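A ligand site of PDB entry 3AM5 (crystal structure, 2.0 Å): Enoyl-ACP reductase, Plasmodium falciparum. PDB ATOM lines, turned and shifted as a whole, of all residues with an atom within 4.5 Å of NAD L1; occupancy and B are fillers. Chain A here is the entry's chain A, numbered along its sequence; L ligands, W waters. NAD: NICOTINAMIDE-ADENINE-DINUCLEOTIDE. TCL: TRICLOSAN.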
ATOM      1  N   GLY A   9     -14.692  -3.034  26.539  1.00  0.00           N
ATOM      2  CA  GLY A   9     -13.368  -2.391  26.408  1.00  0.00           C
ATOM      3  C   GLY A   9     -12.183  -3.348  26.380  1.00  0.00           C
ATOM      4  O   GLY A   9     -11.248  -3.232  27.178  1.00  0.00           O
ATOM      5  N   ILE A  10     -12.217  -4.318  25.484  1.00  0.00           N
ATOM      6  CA  ILE A  10     -11.114  -5.250  25.230  1.00  0.00           C
ATOM      7  C   ILE A  10     -10.742  -5.028  23.761  1.00  0.00           C
ATOM      8  O   ILE A  10     -11.619  -4.999  22.898  1.00  0.00           O
ATOM      9  CB  ILE A  10     -11.540  -6.714  25.511  1.00  0.00           C
ATOM     10  CG1 ILE A  10     -11.362  -7.015  27.004  1.00  0.00           C
ATOM     11  CG2 ILE A  10     -10.691  -7.729  24.730  1.00  0.00           C
ATOM     12  CD1 ILE A  10     -11.992  -8.331  27.494  1.00  0.00           C
ATOM     13  N   GLY A  11      -9.452  -4.807  23.490  1.00  0.00           N
ATOM     14  CA  GLY A  11      -8.951  -4.604  22.129  1.00  0.00           C
ATOM     15  C   GLY A  11      -7.823  -5.571  21.766  1.00  0.00           C
ATOM     16  O   GLY A  11      -7.513  -5.749  20.589  1.00  0.00           O
ATOM     17  N   ASP A  12      -7.235  -6.191  22.772  1.00  0.00           N
ATOM     18  CA  ASP A  12      -6.121  -7.087  22.621  1.00  0.00           C
ATOM     19  C   ASP A  12      -5.909  -7.718  24.021  1.00  0.00           C
ATOM     20  O   ASP A  12      -6.772  -7.598  24.877  1.00  0.00           O
ATOM     21  CB  ASP A  12      -4.892  -6.268  22.254  1.00  0.00           C
ATOM     22  CG  ASP A  12      -4.645  -5.138  23.244  1.00  0.00           C
ATOM     23  OD1 ASP A  12      -4.567  -3.992  22.798  1.00  0.00           O
ATOM     24  OD2 ASP A  12      -4.584  -5.377  24.463  1.00  0.00           O
ATOM     25  N   GLY A  15      -4.320  -5.232  28.002  1.00  0.00           N
ATOM     26  CA  GLY A  15      -4.980  -4.285  28.896  1.00  0.00           C
ATOM     27  C   GLY A  15      -5.583  -4.916  30.144  1.00  0.00           C
ATOM     28  O   GLY A  15      -5.447  -6.126  30.362  1.00  0.00           O
ATOM     29  N   TYR A  16      -6.258  -4.095  30.941  1.00  0.00           N
ATOM     30  CA  TYR A  16      -6.934  -4.592  32.144  1.00  0.00           C
ATOM     31  C   TYR A  16      -8.155  -5.454  31.813  1.00  0.00           C
ATOM     32  O   TYR A  16      -8.446  -6.366  32.536  1.00  0.00           O
ATOM     33  CB  TYR A  16      -7.313  -3.424  33.071  1.00  0.00           C
ATOM     34  CG  TYR A  16      -6.095  -2.933  33.864  1.00  0.00           C
ATOM     35  CD1 TYR A  16      -5.333  -3.831  34.592  1.00  0.00           C
ATOM     36  CD2 TYR A  16      -5.705  -1.576  33.862  1.00  0.00           C
ATOM     37  CE1 TYR A  16      -4.222  -3.433  35.308  1.00  0.00           C
ATOM     38  CE2 TYR A  16      -4.583  -1.158  34.592  1.00  0.00           C
ATOM     39  CZ  TYR A  16      -3.859  -2.098  35.320  1.00  0.00           C
ATOM     40  OH  TYR A  16      -2.739  -1.770  36.057  1.00  0.00           O
ATOM     41  N   GLY A  17      -8.829  -5.185  30.709  1.00  0.00           N
ATOM     42  CA  GLY A  17     -10.023  -5.976  30.351  1.00  0.00           C
ATOM     43  C   GLY A  17      -9.705  -7.472  30.256  1.00  0.00           C
ATOM     44  O   GLY A  17     -10.438  -8.313  30.764  1.00  0.00           O
ATOM     45  N   TRP A  36     -14.520  -2.284  20.602  1.00  0.00           N
ATOM     46  CA  TRP A  36     -14.656  -1.032  19.860  1.00  0.00           C
ATOM     47  C   TRP A  36     -14.606  -1.323  18.354  1.00  0.00           C
ATOM     48  O   TRP A  36     -13.677  -1.978  17.883  1.00  0.00           O
ATOM     49  CB  TRP A  36     -13.524  -0.105  20.285  1.00  0.00           C
ATOM     50  CG  TRP A  36     -13.679   1.307  19.851  1.00  0.00           C
ATOM     51  CD1 TRP A  36     -14.831   2.035  19.806  1.00  0.00           C
ATOM     52  CD2 TRP A  36     -12.627   2.180  19.463  1.00  0.00           C
ATOM     53  NE1 TRP A  36     -14.564   3.317  19.374  1.00  0.00           N
ATOM     54  CE2 TRP A  36     -13.212   3.428  19.166  1.00  0.00           C
ATOM     55  CE3 TRP A  36     -11.239   2.021  19.319  1.00  0.00           C
ATOM     56  CZ2 TRP A  36     -12.447   4.515  18.732  1.00  0.00           C
ATOM     57  CZ3 TRP A  36     -10.486   3.103  18.889  1.00  0.00           C
ATOM     58  CH2 TRP A  36     -11.096   4.342  18.600  1.00  0.00           C
ATOM     59  N   VAL A  39     -11.533  -1.603  15.964  1.00  0.00           N
ATOM     60  CA  VAL A  39     -10.548  -2.692  16.143  1.00  0.00           C
ATOM     61  C   VAL A  39     -11.193  -4.088  16.214  1.00  0.00           C
ATOM     62  O   VAL A  39     -10.519  -5.102  16.499  1.00  0.00           O
ATOM     63  CB  VAL A  39      -9.624  -2.430  17.376  1.00  0.00           C
ATOM     64  CG1 VAL A  39      -9.094  -0.991  17.343  1.00  0.00           C
ATOM     65  CG2 VAL A  39     -10.341  -2.703  18.693  1.00  0.00           C
ATOM     66  N   PHE A  72     -18.981  -2.960  20.036  1.00  0.00           N
ATOM     67  CA  PHE A  72     -19.596  -2.119  21.068  1.00  0.00           C
ATOM     68  C   PHE A  72     -18.919  -0.756  21.032  1.00  0.00           C
ATOM     69  O   PHE A  72     -17.698  -0.666  21.157  1.00  0.00           O
ATOM     70  CB  PHE A  72     -19.412  -2.783  22.441  1.00  0.00           C
ATOM     71  CG  PHE A  72     -19.797  -1.912  23.590  1.00  0.00           C
ATOM     72  CD1 PHE A  72     -21.121  -1.873  24.041  1.00  0.00           C
ATOM     73  CD2 PHE A  72     -18.850  -1.105  24.234  1.00  0.00           C
ATOM     74  CE1 PHE A  72     -21.513  -1.038  25.124  1.00  0.00           C
ATOM     75  CE2 PHE A  72     -19.208  -0.260  25.314  1.00  0.00           C
ATOM     76  CZ  PHE A  72     -20.550  -0.223  25.755  1.00  0.00           C
ATOM     77  N   ASP A  73     -19.701   0.291  20.820  1.00  0.00           N
ATOM     78  CA  ASP A  73     -19.168   1.632  20.828  1.00  0.00           C
ATOM     79  C   ASP A  73     -19.856   2.463  21.895  1.00  0.00           C
ATOM     80  O   ASP A  73     -21.060   2.713  21.807  1.00  0.00           O
ATOM     81  CB  ASP A  73     -19.297   2.299  19.457  1.00  0.00           C
ATOM     82  CG  ASP A  73     -18.468   3.554  19.348  1.00  0.00           C
ATOM     83  OD1 ASP A  73     -18.319   4.267  20.372  1.00  0.00           O
ATOM     84  OD2 ASP A  73     -17.958   3.822  18.243  1.00  0.00           O
ATOM     85  N   ALA A  74     -19.082   2.884  22.894  1.00  0.00           N
ATOM     86  CA  ALA A  74     -19.623   3.562  24.067  1.00  0.00           C
ATOM     87  C   ALA A  74     -19.954   5.028  23.790  1.00  0.00           C
ATOM     88  O   ALA A  74     -20.488   5.704  24.658  1.00  0.00           O
ATOM     89  CB  ALA A  74     -18.652   3.456  25.232  1.00  0.00           C
ATOM     90  N   SER A  75     -19.618   5.512  22.595  1.00  0.00           N
ATOM     91  CA  SER A  75     -19.977   6.860  22.113  1.00  0.00           C
ATOM     92  C   SER A  75     -21.487   7.017  21.872  1.00  0.00           C
ATOM     93  O   SER A  75     -22.004   8.146  21.919  1.00  0.00           O
ATOM     94  CB  SER A  75     -19.335   7.155  20.760  1.00  0.00           C
ATOM     95  OG  SER A  75     -17.950   6.992  20.802  1.00  0.00           O
ATOM     96  N   SER A 120     -14.380  -1.086  31.094  1.00  0.00           N
ATOM     97  CA  SER A 120     -12.926  -1.055  31.062  1.00  0.00           C
ATOM     98  C   SER A 120     -12.470  -0.268  29.841  1.00  0.00           C
ATOM     99  O   SER A 120     -11.778  -0.793  28.979  1.00  0.00           O
ATOM    100  CB  SER A 120     -12.366  -2.491  31.030  1.00  0.00           C
ATOM    101  OG  SER A 120     -10.955  -2.469  31.199  1.00  0.00           O
ATOM    102  N   LEU A 121     -12.885   0.970  29.769  1.00  0.00           N
ATOM    103  CA  LEU A 121     -12.647   1.739  28.583  1.00  0.00           C
ATOM    104  C   LEU A 121     -12.497   3.218  28.916  1.00  0.00           C
ATOM    105  O   LEU A 121     -13.053   3.693  29.923  1.00  0.00           O
ATOM    106  CB  LEU A 121     -13.781   1.517  27.556  1.00  0.00           C
ATOM    107  CG  LEU A 121     -15.203   2.019  27.858  1.00  0.00           C
ATOM    108  CD1 LEU A 121     -15.379   3.416  27.314  1.00  0.00           C
ATOM    109  CD2 LEU A 121     -16.280   1.075  27.261  1.00  0.00           C
ATOM    110  N   ALA A 122     -11.786   3.916  28.040  1.00  0.00           N
ATOM    111  CA  ALA A 122     -11.628   5.368  28.117  1.00  0.00           C
ATOM    112  C   ALA A 122     -11.153   5.861  26.776  1.00  0.00           C
ATOM    113  O   ALA A 122     -10.524   5.121  26.028  1.00  0.00           O
ATOM    114  CB  ALA A 122     -10.641   5.749  29.195  1.00  0.00           C
ATOM    115  N   ASN A 123     -11.496   7.106  26.469  1.00  0.00           N
ATOM    116  CA  ASN A 123     -11.000   7.783  25.287  1.00  0.00           C
ATOM    117  C   ASN A 123     -11.079   9.290  25.530  1.00  0.00           C
ATOM    118  O   ASN A 123     -11.855   9.754  26.374  1.00  0.00           O
ATOM    119  CB  ASN A 123     -11.834   7.400  24.041  1.00  0.00           C
ATOM    120  CG  ASN A 123     -10.972   7.190  22.804  1.00  0.00           C
ATOM    121  OD1 ASN A 123     -11.363   6.440  21.891  1.00  0.00           O
ATOM    122  ND2 ASN A 123      -9.795   7.840  22.763  1.00  0.00           N
ATOM    123  N   LYS A 145     -16.943   9.752  26.457  1.00  0.00           N
ATOM    124  CA  LYS A 145     -16.478   8.393  26.192  1.00  0.00           C
ATOM    125  C   LYS A 145     -16.060   7.661  27.475  1.00  0.00           C
ATOM    126  O   LYS A 145     -16.236   6.443  27.574  1.00  0.00           O
ATOM    127  CB  LYS A 145     -15.304   8.431  25.213  1.00  0.00           C
ATOM    128  CG  LYS A 145     -15.646   8.535  23.715  1.00  0.00           C
ATOM    129  CD  LYS A 145     -16.840   9.383  23.385  1.00  0.00           C
ATOM    130  CE  LYS A 145     -17.033   9.542  21.848  1.00  0.00           C
ATOM    131  NZ  LYS A 145     -15.749   9.705  21.020  1.00  0.00           N
ATOM    132  N   LEU A 170     -12.841   1.102  35.855  1.00  0.00           N
ATOM    133  CA  LEU A 170     -11.460   1.337  36.186  1.00  0.00           C
ATOM    134  C   LEU A 170     -11.215   2.854  36.164  1.00  0.00           C
ATOM    135  O   LEU A 170     -11.728   3.596  35.291  1.00  0.00           O
ATOM    136  CB  LEU A 170     -10.534   0.632  35.173  1.00  0.00           C
ATOM    137  CG  LEU A 170     -10.592  -0.906  35.257  1.00  0.00           C
ATOM    138  CD1 LEU A 170     -10.032  -1.502  34.046  1.00  0.00           C
ATOM    139  CD2 LEU A 170      -9.823  -1.427  36.458  1.00  0.00           C
ATOM    140  N   THR A 171     -10.441   3.307  37.131  1.00  0.00           N
ATOM    141  CA  THR A 171     -10.105   4.718  37.223  1.00  0.00           C
ATOM    142  C   THR A 171      -8.596   4.883  37.474  1.00  0.00           C
ATOM    143  O   THR A 171      -7.823   3.918  37.482  1.00  0.00           O
ATOM    144  CB  THR A 171     -10.999   5.440  38.280  1.00  0.00           C
ATOM    145  OG1 THR A 171     -10.749   6.853  38.251  1.00  0.00           O
ATOM    146  CG2 THR A 171     -10.716   4.882  39.719  1.00  0.00           C
ATOM    147  N   TYR A 172      -8.165   6.109  37.692  1.00  0.00           N
ATOM    148  CA  TYR A 172      -6.760   6.366  37.902  1.00  0.00           C
ATOM    149  C   TYR A 172      -6.620   7.569  38.840  1.00  0.00           C
ATOM    150  O   TYR A 172      -7.451   8.495  38.801  1.00  0.00           O
ATOM    151  CB  TYR A 172      -6.056   6.589  36.557  1.00  0.00           C
ATOM    152  CG  TYR A 172      -4.551   6.875  36.694  1.00  0.00           C
ATOM    153  CD1 TYR A 172      -3.696   5.942  37.271  1.00  0.00           C
ATOM    154  CD2 TYR A 172      -4.004   8.056  36.179  1.00  0.00           C
ATOM    155  CE1 TYR A 172      -2.342   6.187  37.405  1.00  0.00           C
ATOM    156  CE2 TYR A 172      -2.614   8.308  36.285  1.00  0.00           C
ATOM    157  CZ  TYR A 172      -1.808   7.378  36.913  1.00  0.00           C
ATOM    158  OH  TYR A 172      -0.441   7.612  37.024  1.00  0.00           O
ATOM    159  N   TYR A 182      -1.246  13.460  32.112  1.00  0.00           N
ATOM    160  CA  TYR A 182      -2.563  12.797  31.966  1.00  0.00           C
ATOM    161  C   TYR A 182      -3.546  13.866  31.497  1.00  0.00           C
ATOM    162  O   TYR A 182      -4.306  14.408  32.311  1.00  0.00           O
ATOM    163  CB  TYR A 182      -2.985  12.179  33.300  1.00  0.00           C
ATOM    164  CG  TYR A 182      -4.044  11.096  33.240  1.00  0.00           C
ATOM    165  CD1 TYR A 182      -3.771   9.850  32.679  1.00  0.00           C
ATOM    166  CD2 TYR A 182      -5.324  11.323  33.757  1.00  0.00           C
ATOM    167  CE1 TYR A 182      -4.756   8.850  32.630  1.00  0.00           C
ATOM    168  CE2 TYR A 182      -6.310  10.360  33.723  1.00  0.00           C
ATOM    169  CZ  TYR A 182      -6.019   9.117  33.171  1.00  0.00           C
ATOM    170  OH  TYR A 182      -6.999   8.146  33.171  1.00  0.00           O
ATOM    171  N   LYS A 190     -11.998  11.016  34.989  1.00  0.00           N
ATOM    172  CA  LYS A 190     -11.828  10.055  36.085  1.00  0.00           C
ATOM    173  C   LYS A 190     -12.413  10.577  37.406  1.00  0.00           C
ATOM    174  O   LYS A 190     -12.932   9.798  38.190  1.00  0.00           O
ATOM    175  CB  LYS A 190     -10.367   9.643  36.264  1.00  0.00           C
ATOM    176  CG  LYS A 190      -9.781   8.783  35.092  1.00  0.00           C
ATOM    177  CD  LYS A 190     -10.732   7.602  34.708  1.00  0.00           C
ATOM    178  CE  LYS A 190      -9.989   6.599  33.755  1.00  0.00           C
ATOM    179  NZ  LYS A 190     -10.862   5.435  33.390  1.00  0.00           N
ATOM    180  N   ALA A 217      -6.465   1.642  39.327  1.00  0.00           N
ATOM    181  CA  ALA A 217      -5.338   0.780  39.008  1.00  0.00           C
ATOM    182  C   ALA A 217      -4.034   1.580  38.878  1.00  0.00           C
ATOM    183  O   ALA A 217      -4.049   2.736  38.455  1.00  0.00           O
ATOM    184  CB  ALA A 217      -5.622   0.056  37.719  1.00  0.00           C
ATOM    185  N   GLY A 218      -2.916   0.936  39.215  1.00  0.00           N
ATOM    186  CA  GLY A 218      -1.598   1.479  38.874  1.00  0.00           C
ATOM    187  C   GLY A 218      -1.277   1.267  37.393  1.00  0.00           C
ATOM    188  O   GLY A 218      -2.092   0.726  36.641  1.00  0.00           O
ATOM    189  N   PRO A 219      -0.053   1.671  36.961  1.00  0.00           N
ATOM    190  CA  PRO A 219       0.200   1.718  35.527  1.00  0.00           C
ATOM    191  C   PRO A 219       0.475   0.332  34.930  1.00  0.00           C
ATOM    192  O   PRO A 219       1.079  -0.522  35.583  1.00  0.00           O
ATOM    193  CB  PRO A 219       1.423   2.641  35.414  1.00  0.00           C
ATOM    194  CG  PRO A 219       2.162   2.438  36.752  1.00  0.00           C
ATOM    195  CD  PRO A 219       1.127   2.026  37.772  1.00  0.00           C
ATOM    196  N   LEU A 220      -0.032   0.137  33.724  1.00  0.00           N
ATOM    197  CA  LEU A 220       0.172  -1.079  32.933  1.00  0.00           C
ATOM    198  C   LEU A 220       0.423  -0.640  31.492  1.00  0.00           C
ATOM    199  O   LEU A 220      -0.223   0.323  31.009  1.00  0.00           O
ATOM    200  CB  LEU A 220      -1.077  -1.967  32.979  1.00  0.00           C
ATOM    201  CG  LEU A 220      -1.116  -3.297  32.230  1.00  0.00           C
ATOM    202  CD1 LEU A 220      -0.368  -4.350  33.026  1.00  0.00           C
ATOM    203  CD2 LEU A 220      -2.560  -3.700  32.000  1.00  0.00           C
ATOM    204  N   SER A 222      -0.519  -1.045  28.562  1.00  0.00           N
ATOM    205  CA  SER A 222      -1.579  -1.390  27.620  1.00  0.00           C
ATOM    206  C   SER A 222      -1.454  -0.557  26.330  1.00  0.00           C
ATOM    207  O   SER A 222      -0.636   0.397  26.273  1.00  0.00           O
ATOM    208  CB  SER A 222      -2.913  -1.078  28.267  1.00  0.00           C
ATOM    209  OG  SER A 222      -2.996   0.329  28.477  1.00  0.00           O
ATOM    210  N   ARG A 223      -2.266  -0.886  25.317  1.00  0.00           N
ATOM    211  CA  ARG A 223      -2.315  -0.081  24.066  1.00  0.00           C
ATOM    212  C   ARG A 223      -2.598   1.390  24.343  1.00  0.00           C
ATOM    213  O   ARG A 223      -1.834   2.267  23.922  1.00  0.00           O
ATOM    214  CB  ARG A 223      -3.307  -0.664  23.005  1.00  0.00           C
ATOM    215  CG  ARG A 223      -3.272   0.018  21.596  1.00  0.00           C
ATOM    216  CD  ARG A 223      -3.945   1.395  21.575  1.00  0.00           C
ATOM    217  NE  ARG A 223      -4.197   1.983  20.245  1.00  0.00           N
ATOM    218  CZ  ARG A 223      -3.642   3.113  19.794  1.00  0.00           C
ATOM    219  NH1 ARG A 223      -2.770   3.783  20.534  1.00  0.00           N
ATOM    220  NH2 ARG A 223      -3.946   3.576  18.576  1.00  0.00           N
ATOM    221  N   ALA A 224      -3.684   1.673  25.065  1.00  0.00           N
ATOM    222  CA  ALA A 224      -4.067   3.068  25.359  1.00  0.00           C
ATOM    223  C   ALA A 224      -2.979   3.842  26.134  1.00  0.00           C
ATOM    224  O   ALA A 224      -2.714   5.002  25.849  1.00  0.00           O
ATOM    225  CB  ALA A 224      -5.394   3.132  26.078  1.00  0.00           C
ATOM    226  N   ALA A 225      -2.327   3.178  27.091  1.00  0.00           N
ATOM    227  CA  ALA A 225      -1.248   3.801  27.856  1.00  0.00           C
ATOM    228  C   ALA A 225      -0.117   4.359  26.942  1.00  0.00           C
ATOM    229  O   ALA A 225       0.396   5.439  27.216  1.00  0.00           O
ATOM    230  CB  ALA A 225      -0.690   2.820  28.880  1.00  0.00           C
ATOM    231  N   ILE A 274       4.004   6.225  30.124  1.00  0.00           N
ATOM    232  CA  ILE A 274       3.743   4.970  30.829  1.00  0.00           C
ATOM    233  C   ILE A 274       5.051   4.290  31.247  1.00  0.00           C
ATOM    234  O   ILE A 274       5.077   3.632  32.281  1.00  0.00           O
ATOM    235  CB  ILE A 274       2.797   4.001  30.044  1.00  0.00           C
ATOM    236  CG1 ILE A 274       2.125   3.020  31.027  1.00  0.00           C
ATOM    237  CG2 ILE A 274       3.512   3.297  28.868  1.00  0.00           C
ATOM    238  CD1 ILE A 274       1.160   3.717  32.030  1.00  0.00           C
HETATM  239  PA  NAD L   1      -6.664  -0.779  26.734  1.00  0.00           P
HETATM  240  O1A NAD L   1      -6.391  -0.127  25.395  1.00  0.00           O
HETATM  241  O2A NAD L   1      -6.254  -2.212  26.978  1.00  0.00           O
HETATM  242  O5B NAD L   1      -8.245  -0.654  27.024  1.00  0.00           O
HETATM  243  C5B NAD L   1      -8.984   0.475  26.548  1.00  0.00           C
HETATM  244  C4B NAD L   1     -10.052  -0.024  25.571  1.00  0.00           C
HETATM  245  O4B NAD L   1     -11.134   0.911  25.447  1.00  0.00           O
HETATM  246  C3B NAD L   1      -9.490  -0.225  24.168  1.00  0.00           C
HETATM  247  O3B NAD L   1      -9.504  -1.610  23.831  1.00  0.00           O
HETATM  248  C2B NAD L   1     -10.428   0.532  23.241  1.00  0.00           C
HETATM  249  O2B NAD L   1     -10.783  -0.283  22.116  1.00  0.00           O
HETATM  250  C1B NAD L   1     -11.636   0.809  24.118  1.00  0.00           C
HETATM  251  N9A NAD L   1     -12.381   2.008  23.658  1.00  0.00           N
HETATM  252  C8A NAD L   1     -11.884   3.233  23.411  1.00  0.00           C
HETATM  253  N7A NAD L   1     -12.892   4.035  23.014  1.00  0.00           N
HETATM  254  C5A NAD L   1     -14.035   3.301  23.010  1.00  0.00           C
HETATM  255  C6A NAD L   1     -15.456   3.565  22.678  1.00  0.00           C
HETATM  256  N6A NAD L   1     -15.870   4.787  22.270  1.00  0.00           N
HETATM  257  N1A NAD L   1     -16.331   2.543  22.797  1.00  0.00           N
HETATM  258  C2A NAD L   1     -15.917   1.334  23.199  1.00  0.00           C
HETATM  259  N3A NAD L   1     -14.637   1.083  23.497  1.00  0.00           N
HETATM  260  C4A NAD L   1     -13.690   2.028  23.412  1.00  0.00           C
HETATM  261  O3  NAD L   1      -6.032   0.140  27.886  1.00  0.00           O
HETATM  262  PN  NAD L   1      -6.322  -0.183  29.443  1.00  0.00           P
HETATM  263  O1N NAD L   1      -5.216   0.440  30.266  1.00  0.00           O
HETATM  264  O2N NAD L   1      -6.624  -1.651  29.566  1.00  0.00           O
HETATM  265  O5D NAD L   1      -7.677   0.634  29.734  1.00  0.00           O
HETATM  266  C5D NAD L   1      -8.726   0.010  30.479  1.00  0.00           C
HETATM  267  C4D NAD L   1      -9.193   0.943  31.595  1.00  0.00           C
HETATM  268  O4D NAD L   1      -8.266   0.921  32.695  1.00  0.00           O
HETATM  269  C3D NAD L   1      -9.281   2.389  31.112  1.00  0.00           C
HETATM  270  O3D NAD L   1     -10.533   2.942  31.511  1.00  0.00           O
HETATM  271  C2D NAD L   1      -8.163   3.109  31.842  1.00  0.00           C
HETATM  272  O2D NAD L   1      -8.538   4.457  32.154  1.00  0.00           O
HETATM  273  C1D NAD L   1      -7.986   2.276  33.091  1.00  0.00           C
HETATM  274  N1N NAD L   1      -6.655   2.441  33.674  1.00  0.00           N
HETATM  275  C2N NAD L   1      -5.548   2.061  33.002  1.00  0.00           C
HETATM  276  C3N NAD L   1      -4.276   2.221  33.546  1.00  0.00           C
HETATM  277  C7N NAD L   1      -3.061   1.792  32.783  1.00  0.00           C
HETATM  278  O7N NAD L   1      -1.959   2.141  33.191  1.00  0.00           O
HETATM  279  N7N NAD L   1      -3.198   1.058  31.696  1.00  0.00           N
HETATM  280  C4N NAD L   1      -4.086   2.827  34.919  1.00  0.00           C
HETATM  281  C5N NAD L   1      -5.351   3.193  35.526  1.00  0.00           C
HETATM  282  C6N NAD L   1      -6.569   2.980  34.889  1.00  0.00           C
HETATM  283  C1  TCL L   2      -4.132   5.658  33.077  1.00  0.00           C
HETATM  284  C2  TCL L   2      -2.853   5.205  32.733  1.00  0.00           C
HETATM  285  C6  TCL L   2      -5.174   5.461  32.196  1.00  0.00           C
HETATM  286  C5  TCL L   2      -4.897   4.737  30.933  1.00  0.00           C
HETATM  287  C4  TCL L   2      -3.609   4.300  30.611  1.00  0.00           C
HETATM  288  C3  TCL L   2      -2.591   4.545  31.526  1.00  0.00           C
HETATM  289  C11 TCL L   2      -6.826   7.365  27.242  1.00  0.00           C
HETATM  290  C10 TCL L   2      -7.493   6.141  27.155  1.00  0.00           C
HETATM  291  C9  TCL L   2      -7.168   5.200  28.116  1.00  0.00           C
HETATM  292  C8  TCL L   2      -6.188   5.526  29.155  1.00  0.00           C
HETATM  293  C12 TCL L   2      -5.896   7.707  28.218  1.00  0.00           C
HETATM  294  C13 TCL L   2      -5.565   6.776  29.187  1.00  0.00           C
HETATM  295  O7  TCL L   2      -5.920   4.542  30.061  1.00  0.00           O
HETATM  296 CL14 TCL L   2      -1.542   5.497  33.905  1.00  0.00          CL
HETATM  297 CL15 TCL L   2      -7.245   8.550  26.002  1.00  0.00          CL
HETATM  298 CL16 TCL L   2      -7.913   3.583  28.106  1.00  0.00          CL
HETATM  299  O17 TCL L   2      -6.427   5.912  32.468  1.00  0.00           O
HETATM  300  O   HOH W   1     -13.166   2.221  32.944  1.00  0.00           O
HETATM  301  O   HOH W   2     -14.416   7.122  21.023  1.00  0.00           O
HETATM  302  O   HOH W   3      -6.667   1.744  23.115  1.00  0.00           O
HETATM  303  O   HOH W   4     -12.268  -2.532  22.596  1.00  0.00           O
HETATM  304  O   HOH W   5      -3.922  -3.099  25.702  1.00  0.00           O
HETATM  305  O   HOH W   6      -7.557  -4.253  25.473  1.00  0.00           O
HETATM  306  O   HOH W   7      -9.033  -3.038  28.865  1.00  0.00           O
HETATM  307  O   HOH W   8      -8.178  -0.348  21.095  1.00  0.00           O
HETATM  308  O   HOH W   9      -6.588  -2.308  23.499  1.00  0.00           O
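Residues that only touch NAD L1: Gly 9 (3.8 Å), Ile 10 (3.6 Å), Gly 15 (3.1 Å), Trp 36 (3.3 Å), Phe 72 (3.4 Å), Ser 120 (3.4 Å), Ala 122 (3.5 Å), Leu 170 (3.3 Å), Thr 171 (3.0 Å), Tyr 172 (3.6 Å), Ala 217 (3.2 Å), Gly 218 (3.4 Å), Pro 219 (3.2 Å), Arg 223 (3.9 Å) and Ile 274 (3.7 Å). Hydrophobic or aromatic side chains within 4 Å of NAD L1: Tyr 16, Trp 36, Phe 72, Ala 74, Leu 121, Ala 122, Leu 170, Tyr 172, Ala 217, Leu 220, Ala 224 and Ile 274. Of the 32 residues printed, 26 come within 4 Å of NAD L1. The nearest printed residue that does not touch NAD L1 is Lys 145 (4.02 Å).
O2D of NAD L1 lies within hydrogen-bond range of O17 of TCL L2 (2.6 Å).
Water W4 lies within hydrogen-bond range of O of Ile 10, O2B of NAD L1 and N of Trp 36. Water W5 lies within hydrogen-bond range of OD2 of Asp 12, N of Arg 223, O2A of NAD L1 and N of Gly 15. Water W7 lies within hydrogen-bond range of O of Gly 9 (2.8 Å), N of Gly 17 (2.8 Å), O2N of NAD L1 (2.9 Å) and OG of Ser 120 (3.1 Å). Water W9 bridges the side-chain carboxylate (OD1) of Asp 12 and an oxygen (O1A) of NAD L1. Water W2 lies within hydrogen-bond range of the side-chain amino group of Lys 145 (2.9 Å), a nitrogen (N6A) of NAD L1 (3.0 Å) and the side-chain amide oxygen of Asn 123 (3.2 Å). Water W1 lies within hydrogen-bond range of the backbone carbonyl oxygen (O) of Leu 170, an oxygen (O3D) of NAD L1 and the backbone carbonyl oxygen (O) of Leu 121.
The side-chain amino group (NZ) of Lys 190 sits at hydrogen-bond distance from the backbone carbonyl oxygen (O) of Leu 170 (2.8 Å). The backbone carbonyl oxygen (O) of Gly 218 is in hydrogen-bond range of the side-chain hydroxyl (OH) of Tyr 16, 2.6 Å away. The side-chain hydroxyl (OG) of Ser 222 is in hydrogen-bond range of the backbone NH (N) of Ala 225 (3.2 Å). O of Thr 171 is in hydrogen-bond range of N of Ala 217 (3.2 Å). OG of Ser 75 is in hydrogen-bond range of OD1 of Asp 73, at 2.8 Å. OG of Ser 120 lies within hydrogen-bond range of N of Gly 17, at 3.5 Å.
A nitrogen (N1A) of NAD L1 sits at hydrogen-bond distance from the backbone NH of Ala 74, at 2.8 Å. The side-chain amino group of Lys 190 lies within hydrogen-bond range of an oxygen (O2D) of NAD L1, 2.8 Å away. An oxygen (O2N) of NAD L1 lies within hydrogen-bond range of the backbone NH (N) of Tyr 16 (2.8 Å). O7N of NAD L1 lies within hydrogen-bond range of N of Leu 220. The backbone carbonyl oxygen (O) of Leu 220 lies within hydrogen-bond range of a nitrogen (N7N) of NAD L1, at 3.1 Å. An oxygen (O1N) of NAD L1 sits at hydrogen-bond distance from the side-chain hydroxyl (OG) of Ser 222, at 2.9 Å. OD1 of Asn 123 lies close to N7A of NAD L1 (3.1 Å). An oxygen (O3D) of NAD L1 is in hydrogen-bond range of the backbone carbonyl oxygen (O) of Leu 121 (3.1 Å). The side-chain carboxylate (OD1) of Asp 73 sits at hydrogen-bond distance from a nitrogen (N6A) of NAD L1 (3.1 Å). N of Gly 11 is in hydrogen-bond range of O3B of NAD L1 (3.2 Å). The backbone NH (N) of Ala 224 sits at hydrogen-bond distance from an oxygen (O1A) of NAD L1, 3.3 Å away. The side-chain hydroxyl (OG) of Ser 75 sits at hydrogen-bond distance from a nitrogen (N6A) of NAD L1 (3.4 Å). O17 of TCL L2 is in hydrogen-bond range of OH of Tyr 182 (2.4 Å).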
